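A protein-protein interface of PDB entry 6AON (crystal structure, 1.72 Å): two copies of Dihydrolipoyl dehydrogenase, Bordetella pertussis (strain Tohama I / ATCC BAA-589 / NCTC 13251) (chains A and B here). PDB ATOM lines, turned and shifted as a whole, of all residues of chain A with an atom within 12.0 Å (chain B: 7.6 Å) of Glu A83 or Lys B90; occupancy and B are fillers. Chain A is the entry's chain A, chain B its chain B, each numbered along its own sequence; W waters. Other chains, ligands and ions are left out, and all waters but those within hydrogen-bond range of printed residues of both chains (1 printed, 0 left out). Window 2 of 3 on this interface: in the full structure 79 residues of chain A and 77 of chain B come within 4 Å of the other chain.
Of chain B, only Gly B86 (3.96 Å), Val B87 (3.5 Å), Ser B88 (3.0 Å) and Lys B90 (2.7 Å) come within 4 Å of Glu A83. Of the printed residues of chain A, Lys B90 touches Gly A81 and Glu A83. Printed residues of chain A within 4 Å of Gly B86: Glu A83, Val A84 and Lys A85. Leu B89 touches just one residue of chain A: Gly A81 (3.5 Å). Of chain A, only Ala A78 (3.8 Å), Glu A79 (3.7 Å) and Gly A81 (3.8 Å) come within 4 Å of Thr B93. Of the printed residues of chain B, Glu A79 touches Thr B93. Printed residues of chain B within 4 Å of Gly A81: Ser B88, Leu B89, Lys B90 and Thr B93. Of the printed residues of chain B, Phe A77 touches Ala B73. Ala A73 touches none of the printed residues of chain B. Glu A71 touches none of the printed residues of chain B. The nearest residue of chain B that does not touch Glu A83 is Leu B89 (5.1 Å).
Of the 19 printed residues of chain A, 9 touch a printed residue of chain B. Among the printed residues, Asp or Glu carboxylates within 4 Å of a Lys or Arg side-chain nitrogen of the other chain: Glu A83 with Lys B90 (2.7 Å).
Among the printed residues, pairs that only touch across the chains: His A80 with Leu B94 (3.2 Å), Ile A82 with Tyr B70 (3.3 Å), Val A84 with Gly B86 (3.4 Å), Glu A83 with Val B87 (3.5 Å), Gly A81 with Leu B89 (3.5 Å), Glu A79 with Thr B93 (3.7 Å), Ala A78 with Thr B93 (3.8 Å), Phe A77 with Ala B73 (3.8 Å), Gly A81 with Thr B93 (3.8 Å), Ile A82 with Ser B88 (3.8 Å), Gly A81 with Ser B88 (3.9 Å), Glu A83 with Gly B86 (3.96 Å) and Val A84 with Val B87 (3.99 Å).
O of Gln A72 sits at hydrogen-bond distance from N of Phe A77 (3.1 Å). The backbone carbonyl oxygen (O) of Phe A77 sits at hydrogen-bond distance from the backbone NH (N) of Ile A82.
Water W1 bridges O of Glu A83 (2.7 Å) and OG of Ser B88 (3.4 Å).
N of Glu A83 is in hydrogen-bond range of O of Ser B88 (3.0 Å). The side-chain amino group (NZ) of Lys B90 lies within salt-bridge range of the side-chain carboxylate (OE1) of Glu A83 (2.7 Å). The backbone carbonyl oxygen of Gly B86 is in hydrogen-bond range of the backbone NH of Lys A85 (3.1 Å). The backbone NH (N) of Lys B90 is in hydrogen-bond range of the backbone carbonyl oxygen (O) of Gly A81 (2.8 Å).
Positions printed for both chains: 70, 73, 86, 87 and 88. Of the 17 pairs that touch across the chains among the printed residues, none has its exchanged pair printed and touching as well.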
ATOM      1  N   TYR A  70      18.043 -23.602  -8.088  1.00  0.00           N
ATOM      2  CA  TYR A  70      18.094 -22.585  -9.141  1.00  0.00           C
ATOM      3  C   TYR A  70      19.533 -22.100  -9.316  1.00  0.00           C
ATOM      4  O   TYR A  70      20.023 -21.983 -10.447  1.00  0.00           O
ATOM      5  CB  TYR A  70      17.119 -21.432  -8.835  1.00  0.00           C
ATOM      6  CG  TYR A  70      16.985 -20.395  -9.935  1.00  0.00           C
ATOM      7  CD1 TYR A  70      16.391 -20.719 -11.154  1.00  0.00           C
ATOM      8  CD2 TYR A  70      17.402 -19.084  -9.738  1.00  0.00           C
ATOM      9  CE1 TYR A  70      16.251 -19.770 -12.159  1.00  0.00           C
ATOM     10  CE2 TYR A  70      17.260 -18.128 -10.729  1.00  0.00           C
ATOM     11  CZ  TYR A  70      16.684 -18.478 -11.936  1.00  0.00           C
ATOM     12  OH  TYR A  70      16.549 -17.531 -12.910  1.00  0.00           O
ATOM     13  N   GLU A  71      20.210 -21.874  -8.191  1.00  0.00           N
ATOM     14  CA  GLU A  71      21.612 -21.448  -8.181  1.00  0.00           C
ATOM     15  C   GLU A  71      22.522 -22.506  -8.810  1.00  0.00           C
ATOM     16  O   GLU A  71      23.417 -22.158  -9.589  1.00  0.00           O
ATOM     17  CB  GLU A  71      22.073 -21.198  -6.744  1.00  0.00           C
ATOM     18  CG  GLU A  71      23.461 -20.599  -6.587  1.00  0.00           C
ATOM     19  CD  GLU A  71      23.471 -19.095  -6.684  1.00  0.00           C
ATOM     20  OE1 GLU A  71      22.737 -18.515  -7.517  1.00  0.00           O
ATOM     21  OE2 GLU A  71      24.226 -18.486  -5.904  1.00  0.00           O
ATOM     22  N   GLN A  72      22.308 -23.773  -8.442  1.00  0.00           N
ATOM     23  CA  GLN A  72      23.071 -24.906  -8.999  1.00  0.00           C
ATOM     24  C   GLN A  72      22.971 -24.950 -10.516  1.00  0.00           C
ATOM     25  O   GLN A  72      23.970 -25.136 -11.212  1.00  0.00           O
ATOM     26  CB  GLN A  72      22.534 -26.257  -8.490  1.00  0.00           C
ATOM     27  CG  GLN A  72      22.834 -26.650  -7.047  1.00  0.00           C
ATOM     28  CD  GLN A  72      22.220 -28.011  -6.658  1.00  0.00           C
ATOM     29  OE1 GLN A  72      21.209 -28.458  -7.227  1.00  0.00           O
ATOM     30  NE2 GLN A  72      22.830 -28.668  -5.676  1.00  0.00           N
ATOM     31  N   ALA A  73      21.748 -24.801 -11.014  1.00  0.00           N
ATOM     32  CA  ALA A  73      21.468 -24.862 -12.450  1.00  0.00           C
ATOM     33  C   ALA A  73      22.187 -23.762 -13.216  1.00  0.00           C
ATOM     34  O   ALA A  73      22.717 -24.002 -14.304  1.00  0.00           O
ATOM     35  CB  ALA A  73      19.974 -24.746 -12.703  1.00  0.00           C
ATOM     36  N   ASN A  74      22.188 -22.561 -12.641  1.00  0.00           N
ATOM     37  CA  ASN A  74      22.825 -21.403 -13.279  1.00  0.00           C
ATOM     38  C   ASN A  74      24.343 -21.398 -13.211  1.00  0.00           C
ATOM     39  O   ASN A  74      24.995 -20.968 -14.175  1.00  0.00           O
ATOM     40  CB  ASN A  74      22.318 -20.091 -12.655  1.00  0.00           C
ATOM     41  CG  ASN A  74      20.908 -19.735 -13.084  1.00  0.00           C
ATOM     42  OD1 ASN A  74      20.598 -19.714 -14.274  1.00  0.00           O
ATOM     43  ND2 ASN A  74      20.061 -19.402 -12.119  1.00  0.00           N
ATOM     44  N   HIS A  75      24.921 -21.889 -12.111  1.00  0.00           N
ATOM     45  CA  HIS A  75      26.375 -21.769 -11.940  1.00  0.00           C
ATOM     46  C   HIS A  75      27.201 -23.019 -11.619  1.00  0.00           C
ATOM     47  O   HIS A  75      28.415 -23.006 -11.831  1.00  0.00           O
ATOM     48  CB  HIS A  75      26.652 -20.730 -10.845  1.00  0.00           C
ATOM     49  CG  HIS A  75      25.923 -19.438 -11.041  1.00  0.00           C
ATOM     50  ND1 HIS A  75      26.224 -18.563 -12.061  1.00  0.00           N
ATOM     51  CD2 HIS A  75      24.918 -18.865 -10.339  1.00  0.00           C
ATOM     52  CE1 HIS A  75      25.427 -17.510 -11.984  1.00  0.00           C
ATOM     53  NE2 HIS A  75      24.630 -17.666 -10.944  1.00  0.00           N
ATOM     54  N   HIS A  76      26.583 -24.088 -11.134  1.00  0.00           N
ATOM     55  CA  HIS A  76      27.375 -25.260 -10.740  1.00  0.00           C
ATOM     56  C   HIS A  76      27.159 -26.534 -11.520  1.00  0.00           C
ATOM     57  O   HIS A  76      27.670 -27.566 -11.138  1.00  0.00           O
ATOM     58  CB  HIS A  76      27.208 -25.499  -9.241  1.00  0.00           C
ATOM     59  CG  HIS A  76      27.708 -24.356  -8.420  1.00  0.00           C
ATOM     60  ND1 HIS A  76      26.866 -23.428  -7.847  1.00  0.00           N
ATOM     61  CD2 HIS A  76      28.968 -23.927  -8.173  1.00  0.00           C
ATOM     62  CE1 HIS A  76      27.587 -22.512  -7.225  1.00  0.00           C
ATOM     63  NE2 HIS A  76      28.866 -22.791  -7.409  1.00  0.00           N
ATOM     64  N   PHE A  77      26.444 -26.465 -12.630  1.00  0.00           N
ATOM     65  CA  PHE A  77      26.203 -27.653 -13.443  1.00  0.00           C
ATOM     66  C   PHE A  77      27.219 -27.776 -14.592  1.00  0.00           C
ATOM     67  O   PHE A  77      27.589 -28.894 -14.960  1.00  0.00           O
ATOM     68  CB  PHE A  77      24.711 -27.702 -13.852  1.00  0.00           C
ATOM     69  CG  PHE A  77      23.804 -28.374 -12.811  1.00  0.00           C
ATOM     70  CD1 PHE A  77      24.158 -28.446 -11.459  1.00  0.00           C
ATOM     71  CD2 PHE A  77      22.555 -28.855 -13.177  1.00  0.00           C
ATOM     72  CE1 PHE A  77      23.328 -29.064 -10.523  1.00  0.00           C
ATOM     73  CE2 PHE A  77      21.717 -29.454 -12.252  1.00  0.00           C
ATOM     74  CZ  PHE A  77      22.096 -29.561 -10.920  1.00  0.00           C
ATOM     75  N   ALA A  78      27.738 -26.654 -15.102  1.00  0.00           N
ATOM     76  CA  ALA A  78      28.739 -26.718 -16.176  1.00  0.00           C
ATOM     77  C   ALA A  78      29.950 -27.566 -15.788  1.00  0.00           C
ATOM     78  O   ALA A  78      30.366 -28.425 -16.559  1.00  0.00           O
ATOM     79  CB  ALA A  78      29.192 -25.322 -16.590  1.00  0.00           C
ATOM     80  N   GLU A  79      30.481 -27.338 -14.586  1.00  0.00           N
ATOM     81  CA  GLU A  79      31.681 -28.059 -14.104  1.00  0.00           C
ATOM     82  C   GLU A  79      31.499 -29.580 -14.006  1.00  0.00           C
ATOM     83  O   GLU A  79      32.469 -30.331 -14.119  1.00  0.00           O
ATOM     84  CB  GLU A  79      32.180 -27.466 -12.779  1.00  0.00           C
ATOM     85  CG  GLU A  79      31.213 -27.585 -11.611  1.00  0.00           C
ATOM     86  CD  GLU A  79      31.554 -26.661 -10.450  1.00  0.00           C
ATOM     87  OE1 GLU A  79      32.073 -25.553 -10.684  1.00  0.00           O
ATOM     88  OE2 GLU A  79      31.253 -27.016  -9.295  1.00  0.00           O
ATOM     89  N   HIS A  80      30.257 -30.020 -13.817  1.00  0.00           N
ATOM     90  CA  HIS A  80      29.923 -31.445 -13.792  1.00  0.00           C
ATOM     91  C   HIS A  80      29.630 -31.998 -15.189  1.00  0.00           C
ATOM     92  O   HIS A  80      29.229 -33.149 -15.320  1.00  0.00           O
ATOM     93  CB  HIS A  80      28.712 -31.687 -12.894  1.00  0.00           C
ATOM     94  CG  HIS A  80      28.994 -31.515 -11.443  1.00  0.00           C
ATOM     95  ND1 HIS A  80      29.347 -32.569 -10.628  1.00  0.00           N
ATOM     96  CD2 HIS A  80      28.953 -30.422 -10.648  1.00  0.00           C
ATOM     97  CE1 HIS A  80      29.518 -32.126  -9.397  1.00  0.00           C
ATOM     98  NE2 HIS A  80      29.283 -30.828  -9.382  1.00  0.00           N
ATOM     99  N   GLY A  81      29.827 -31.185 -16.230  1.00  0.00           N
ATOM    100  CA  GLY A  81      29.574 -31.615 -17.607  1.00  0.00           C
ATOM    101  C   GLY A  81      28.103 -31.586 -17.994  1.00  0.00           C
ATOM    102  O   GLY A  81      27.685 -32.296 -18.917  1.00  0.00           O
ATOM    103  N   ILE A  82      27.325 -30.763 -17.295  1.00  0.00           N
ATOM    104  CA  ILE A  82      25.898 -30.618 -17.560  1.00  0.00           C
ATOM    105  C   ILE A  82      25.659 -29.224 -18.134  1.00  0.00           C
ATOM    106  O   ILE A  82      25.715 -28.232 -17.415  1.00  0.00           O
ATOM    107  CB  ILE A  82      25.075 -30.810 -16.283  1.00  0.00           C
ATOM    108  CG1 ILE A  82      25.396 -32.166 -15.640  1.00  0.00           C
ATOM    109  CG2 ILE A  82      23.582 -30.690 -16.595  1.00  0.00           C
ATOM    110  CD1 ILE A  82      24.843 -32.306 -14.240  1.00  0.00           C
ATOM    111  N   GLU A  83      25.410 -29.163 -19.434  1.00  0.00           N
ATOM    112  CA  GLU A  83      25.174 -27.898 -20.111  1.00  0.00           C
ATOM    113  C   GLU A  83      23.672 -27.637 -20.164  1.00  0.00           C
ATOM    114  O   GLU A  83      22.950 -28.298 -20.914  1.00  0.00           O
ATOM    115  CB  GLU A  83      25.778 -27.937 -21.511  1.00  0.00           C
ATOM    116  CG  GLU A  83      25.550 -26.674 -22.329  1.00  0.00           C
ATOM    117  CD  GLU A  83      26.303 -26.694 -23.644  1.00  0.00           C
ATOM    118  OE1 GLU A  83      27.545 -26.856 -23.619  1.00  0.00           O
ATOM    119  OE2 GLU A  83      25.659 -26.518 -24.700  1.00  0.00           O
ATOM    120  N   VAL A  84      23.211 -26.701 -19.334  1.00  0.00           N
ATOM    121  CA  VAL A  84      21.794 -26.336 -19.280  1.00  0.00           C
ATOM    122  C   VAL A  84      21.629 -24.932 -19.849  1.00  0.00           C
ATOM    123  O   VAL A  84      22.155 -23.967 -19.291  1.00  0.00           O
ATOM    124  CB  VAL A  84      21.215 -26.432 -17.848  1.00  0.00           C
ATOM    125  CG1 VAL A  84      21.464 -27.817 -17.278  1.00  0.00           C
ATOM    126  CG2 VAL A  84      21.797 -25.388 -16.910  1.00  0.00           C
ATOM    127  N   LYS A  85      20.921 -24.827 -20.976  1.00  0.00           N
ATOM    128  CA  LYS A  85      20.712 -23.533 -21.642  1.00  0.00           C
ATOM    129  C   LYS A  85      19.322 -22.934 -21.370  1.00  0.00           C
ATOM    130  O   LYS A  85      18.333 -23.654 -21.231  1.00  0.00           O
ATOM    131  CB  LYS A  85      20.936 -23.670 -23.157  1.00  0.00           C
ATOM    132  CG  LYS A  85      19.854 -24.443 -23.899  1.00  0.00           C
ATOM    133  CD  LYS A  85      20.149 -24.588 -25.381  1.00  0.00           C
ATOM    134  CE  LYS A  85      18.961 -25.204 -26.105  1.00  0.00           C
ATOM    135  NZ  LYS A  85      19.226 -25.377 -27.558  1.00  0.00           N
ATOM    136  N   GLY A  86      19.271 -21.611 -21.289  1.00  0.00           N
ATOM    137  CA  GLY A  86      18.022 -20.880 -21.101  1.00  0.00           C
ATOM    138  C   GLY A  86      17.266 -21.192 -19.830  1.00  0.00           C
ATOM    139  O   GLY A  86      16.090 -21.568 -19.881  1.00  0.00           O
ATOM    140  N   VAL A  87      17.944 -21.041 -18.695  1.00  0.00           N
ATOM    141  CA  VAL A  87      17.341 -21.291 -17.393  1.00  0.00           C
ATOM    142  C   VAL A  87      16.463 -20.100 -17.024  1.00  0.00           C
ATOM    143  O   VAL A  87      16.898 -18.952 -17.118  1.00  0.00           O
ATOM    144  CB  VAL A  87      18.408 -21.493 -16.295  1.00  0.00           C
ATOM    145  CG1 VAL A  87      17.753 -21.754 -14.943  1.00  0.00           C
ATOM    146  CG2 VAL A  87      19.336 -22.637 -16.655  1.00  0.00           C
ATOM    147  N   SER A  88      15.220 -20.373 -16.636  1.00  0.00           N
ATOM    148  CA  SER A  88      14.297 -19.319 -16.218  1.00  0.00           C
ATOM    149  C   SER A  88      13.497 -19.780 -15.004  1.00  0.00           C
ATOM    150  O   SER A  88      13.406 -20.967 -14.720  1.00  0.00           O
ATOM    151  CB  SER A  88      13.378 -18.882 -17.357  1.00  0.00           C
ATOM    152  OG  SER A  88      12.555 -19.944 -17.778  1.00  0.00           O
ATOM    153  N   TYR B  70      22.629 -34.531 -13.154  1.00  0.00           N
ATOM    154  CA  TYR B  70      22.095 -34.645 -14.516  1.00  0.00           C
ATOM    155  C   TYR B  70      20.670 -35.176 -14.476  1.00  0.00           C
ATOM    156  O   TYR B  70      19.802 -34.686 -15.201  1.00  0.00           O
ATOM    157  CB  TYR B  70      22.996 -35.547 -15.364  1.00  0.00           C
ATOM    158  CG  TYR B  70      22.663 -35.595 -16.838  1.00  0.00           C
ATOM    159  CD1 TYR B  70      22.826 -34.477 -17.639  1.00  0.00           C
ATOM    160  CD2 TYR B  70      22.283 -36.787 -17.450  1.00  0.00           C
ATOM    161  CE1 TYR B  70      22.558 -34.526 -18.998  1.00  0.00           C
ATOM    162  CE2 TYR B  70      22.022 -36.847 -18.807  1.00  0.00           C
ATOM    163  CZ  TYR B  70      22.161 -35.709 -19.574  1.00  0.00           C
ATOM    164  OH  TYR B  70      21.914 -35.751 -20.920  1.00  0.00           O
ATOM    165  N   ALA B  73      18.428 -32.325 -13.226  1.00  0.00           N
ATOM    166  CA  ALA B  73      18.219 -31.333 -14.292  1.00  0.00           C
ATOM    167  C   ALA B  73      17.219 -31.804 -15.341  1.00  0.00           C
ATOM    168  O   ALA B  73      16.501 -30.997 -15.921  1.00  0.00           O
ATOM    169  CB  ALA B  73      19.535 -31.001 -14.967  1.00  0.00           C
ATOM    170  N   GLY B  86      16.962 -26.451 -22.594  1.00  0.00           N
ATOM    171  CA  GLY B  86      17.609 -27.693 -22.987  1.00  0.00           C
ATOM    172  C   GLY B  86      18.648 -28.142 -21.986  1.00  0.00           C
ATOM    173  O   GLY B  86      19.119 -27.333 -21.179  1.00  0.00           O
ATOM    174  N   VAL B  87      18.971 -29.438 -22.037  1.00  0.00           N
ATOM    175  CA  VAL B  87      19.979 -30.067 -21.185  1.00  0.00           C
ATOM    176  C   VAL B  87      20.762 -31.052 -22.046  1.00  0.00           C
ATOM    177  O   VAL B  87      20.165 -31.865 -22.751  1.00  0.00           O
ATOM    178  CB  VAL B  87      19.350 -30.845 -20.002  1.00  0.00           C
ATOM    179  CG1 VAL B  87      20.428 -31.586 -19.209  1.00  0.00           C
ATOM    180  CG2 VAL B  87      18.580 -29.907 -19.080  1.00  0.00           C
ATOM    181  N   SER B  88      22.091 -30.954 -22.024  1.00  0.00           N
ATOM    182  CA  SER B  88      22.940 -31.878 -22.784  1.00  0.00           C
ATOM    183  C   SER B  88      24.144 -32.227 -21.943  1.00  0.00           C
ATOM    184  O   SER B  88      24.528 -31.487 -21.038  1.00  0.00           O
ATOM    185  CB  SER B  88      23.371 -31.307 -24.138  1.00  0.00           C
ATOM    186  OG  SER B  88      24.200 -30.178 -23.986  1.00  0.00           O
ATOM    187  N   LEU B  89      24.736 -33.361 -22.268  1.00  0.00           N
ATOM    188  CA  LEU B  89      25.861 -33.888 -21.536  1.00  0.00           C
ATOM    189  C   LEU B  89      27.189 -33.675 -22.243  1.00  0.00           C
ATOM    190  O   LEU B  89      27.305 -33.891 -23.459  1.00  0.00           O
ATOM    191  CB  LEU B  89      25.641 -35.395 -21.356  1.00  0.00           C
ATOM    192  CG  LEU B  89      26.671 -36.198 -20.568  1.00  0.00           C
ATOM    193  CD1 LEU B  89      26.761 -35.669 -19.147  1.00  0.00           C
ATOM    194  CD2 LEU B  89      26.296 -37.673 -20.581  1.00  0.00           C
ATOM    195  N   LYS B  90      28.190 -33.271 -21.466  1.00  0.00           N
ATOM    196  CA  LYS B  90      29.556 -33.130 -21.932  1.00  0.00           C
ATOM    197  C   LYS B  90      30.332 -34.138 -21.110  1.00  0.00           C
ATOM    198  O   LYS B  90      30.900 -33.810 -20.064  1.00  0.00           O
ATOM    199  CB  LYS B  90      30.046 -31.700 -21.742  1.00  0.00           C
ATOM    200  CG  LYS B  90      29.324 -30.741 -22.677  1.00  0.00           C
ATOM    201  CD  LYS B  90      29.789 -30.912 -24.121  1.00  0.00           C
ATOM    202  CE  LYS B  90      28.710 -30.518 -25.116  1.00  0.00           C
ATOM    203  NZ  LYS B  90      28.098 -29.193 -24.832  1.00  0.00           N
ATOM    204  N   LEU B  91      30.324 -35.385 -21.587  1.00  0.00           N
ATOM    205  CA  LEU B  91      30.934 -36.497 -20.851  1.00  0.00           C
ATOM    206  C   LEU B  91      32.416 -36.324 -20.536  1.00  0.00           C
ATOM    207  O   LEU B  91      32.849 -36.719 -19.467  1.00  0.00           O
ATOM    208  CB  LEU B  91      30.669 -37.835 -21.543  1.00  0.00           C
ATOM    209  CG  LEU B  91      31.053 -39.092 -20.750  1.00  0.00           C
ATOM    210  CD1 LEU B  91      30.338 -39.151 -19.408  1.00  0.00           C
ATOM    211  CD2 LEU B  91      30.747 -40.333 -21.572  1.00  0.00           C
ATOM    212  N   ASP B  92      33.180 -35.731 -21.450  1.00  0.00           N
ATOM    213  CA  ASP B  92      34.604 -35.496 -21.212  1.00  0.00           C
ATOM    214  C   ASP B  92      34.834 -34.607 -19.989  1.00  0.00           C
ATOM    215  O   ASP B  92      35.775 -34.826 -19.223  1.00  0.00           O
ATOM    216  CB  ASP B  92      35.266 -34.870 -22.444  1.00  0.00           C
ATOM    217  CG  ASP B  92      35.333 -35.830 -23.630  1.00  0.00           C
ATOM    218  OD1 ASP B  92      35.252 -37.061 -23.426  1.00  0.00           O
ATOM    219  OD2 ASP B  92      35.503 -35.349 -24.762  1.00  0.00           O
ATOM    220  N   THR B  93      33.974 -33.608 -19.811  1.00  0.00           N
ATOM    221  CA  THR B  93      34.079 -32.689 -18.683  1.00  0.00           C
ATOM    222  C   THR B  93      33.674 -33.386 -17.381  1.00  0.00           C
ATOM    223  O   THR B  93      34.305 -33.183 -16.333  1.00  0.00           O
ATOM    224  CB  THR B  93      33.188 -31.461 -18.924  1.00  0.00           C
ATOM    225  OG1 THR B  93      33.609 -30.820 -20.134  1.00  0.00           O
ATOM    226  CG2 THR B  93      33.264 -30.483 -17.762  1.00  0.00           C
ATOM    227  N   LEU B  94      32.625 -34.204 -17.450  1.00  0.00           N
ATOM    228  CA  LEU B  94      32.153 -34.957 -16.276  1.00  0.00           C
ATOM    229  C   LEU B  94      33.237 -35.941 -15.816  1.00  0.00           C
ATOM    230  O   LEU B  94      33.596 -35.960 -14.625  1.00  0.00           O
ATOM    231  CB  LEU B  94      30.819 -35.656 -16.584  1.00  0.00           C
ATOM    232  CG  LEU B  94      30.070 -36.390 -15.457  1.00  0.00           C
ATOM    233  CD1 LEU B  94      28.581 -36.551 -15.757  1.00  0.00           C
ATOM    234  CD2 LEU B  94      30.703 -37.743 -15.133  1.00  0.00           C
ATOM    235  N   ILE B  95      33.769 -36.733 -16.750  1.00  0.00           N
ATOM    236  CA  ILE B  95      34.849 -37.681 -16.433  1.00  0.00           C
ATOM    237  C   ILE B  95      36.111 -36.910 -16.031  1.00  0.00           C
ATOM    238  O   ILE B  95      36.844 -37.324 -15.129  1.00  0.00           O
ATOM    239  CB  ILE B  95      35.155 -38.646 -17.609  1.00  0.00           C
ATOM    240  CG1 ILE B  95      33.929 -39.501 -17.949  1.00  0.00           C
ATOM    241  CG2 ILE B  95      36.347 -39.546 -17.299  1.00  0.00           C
ATOM    242  CD1 ILE B  95      33.365 -40.300 -16.799  1.00  0.00           C
ATOM    243  N   GLY B  96      36.336 -35.766 -16.682  1.00  0.00           N
ATOM    244  CA  GLY B  96      37.490 -34.915 -16.385  1.00  0.00           C
ATOM    245  C   GLY B  96      37.513 -34.387 -14.959  1.00  0.00           C
ATOM    246  O   GLY B  96      38.585 -34.311 -14.352  1.00  0.00           O
HETATM  247  O   HOH W   1      21.910 -27.770 -23.393  1.00  0.00           O
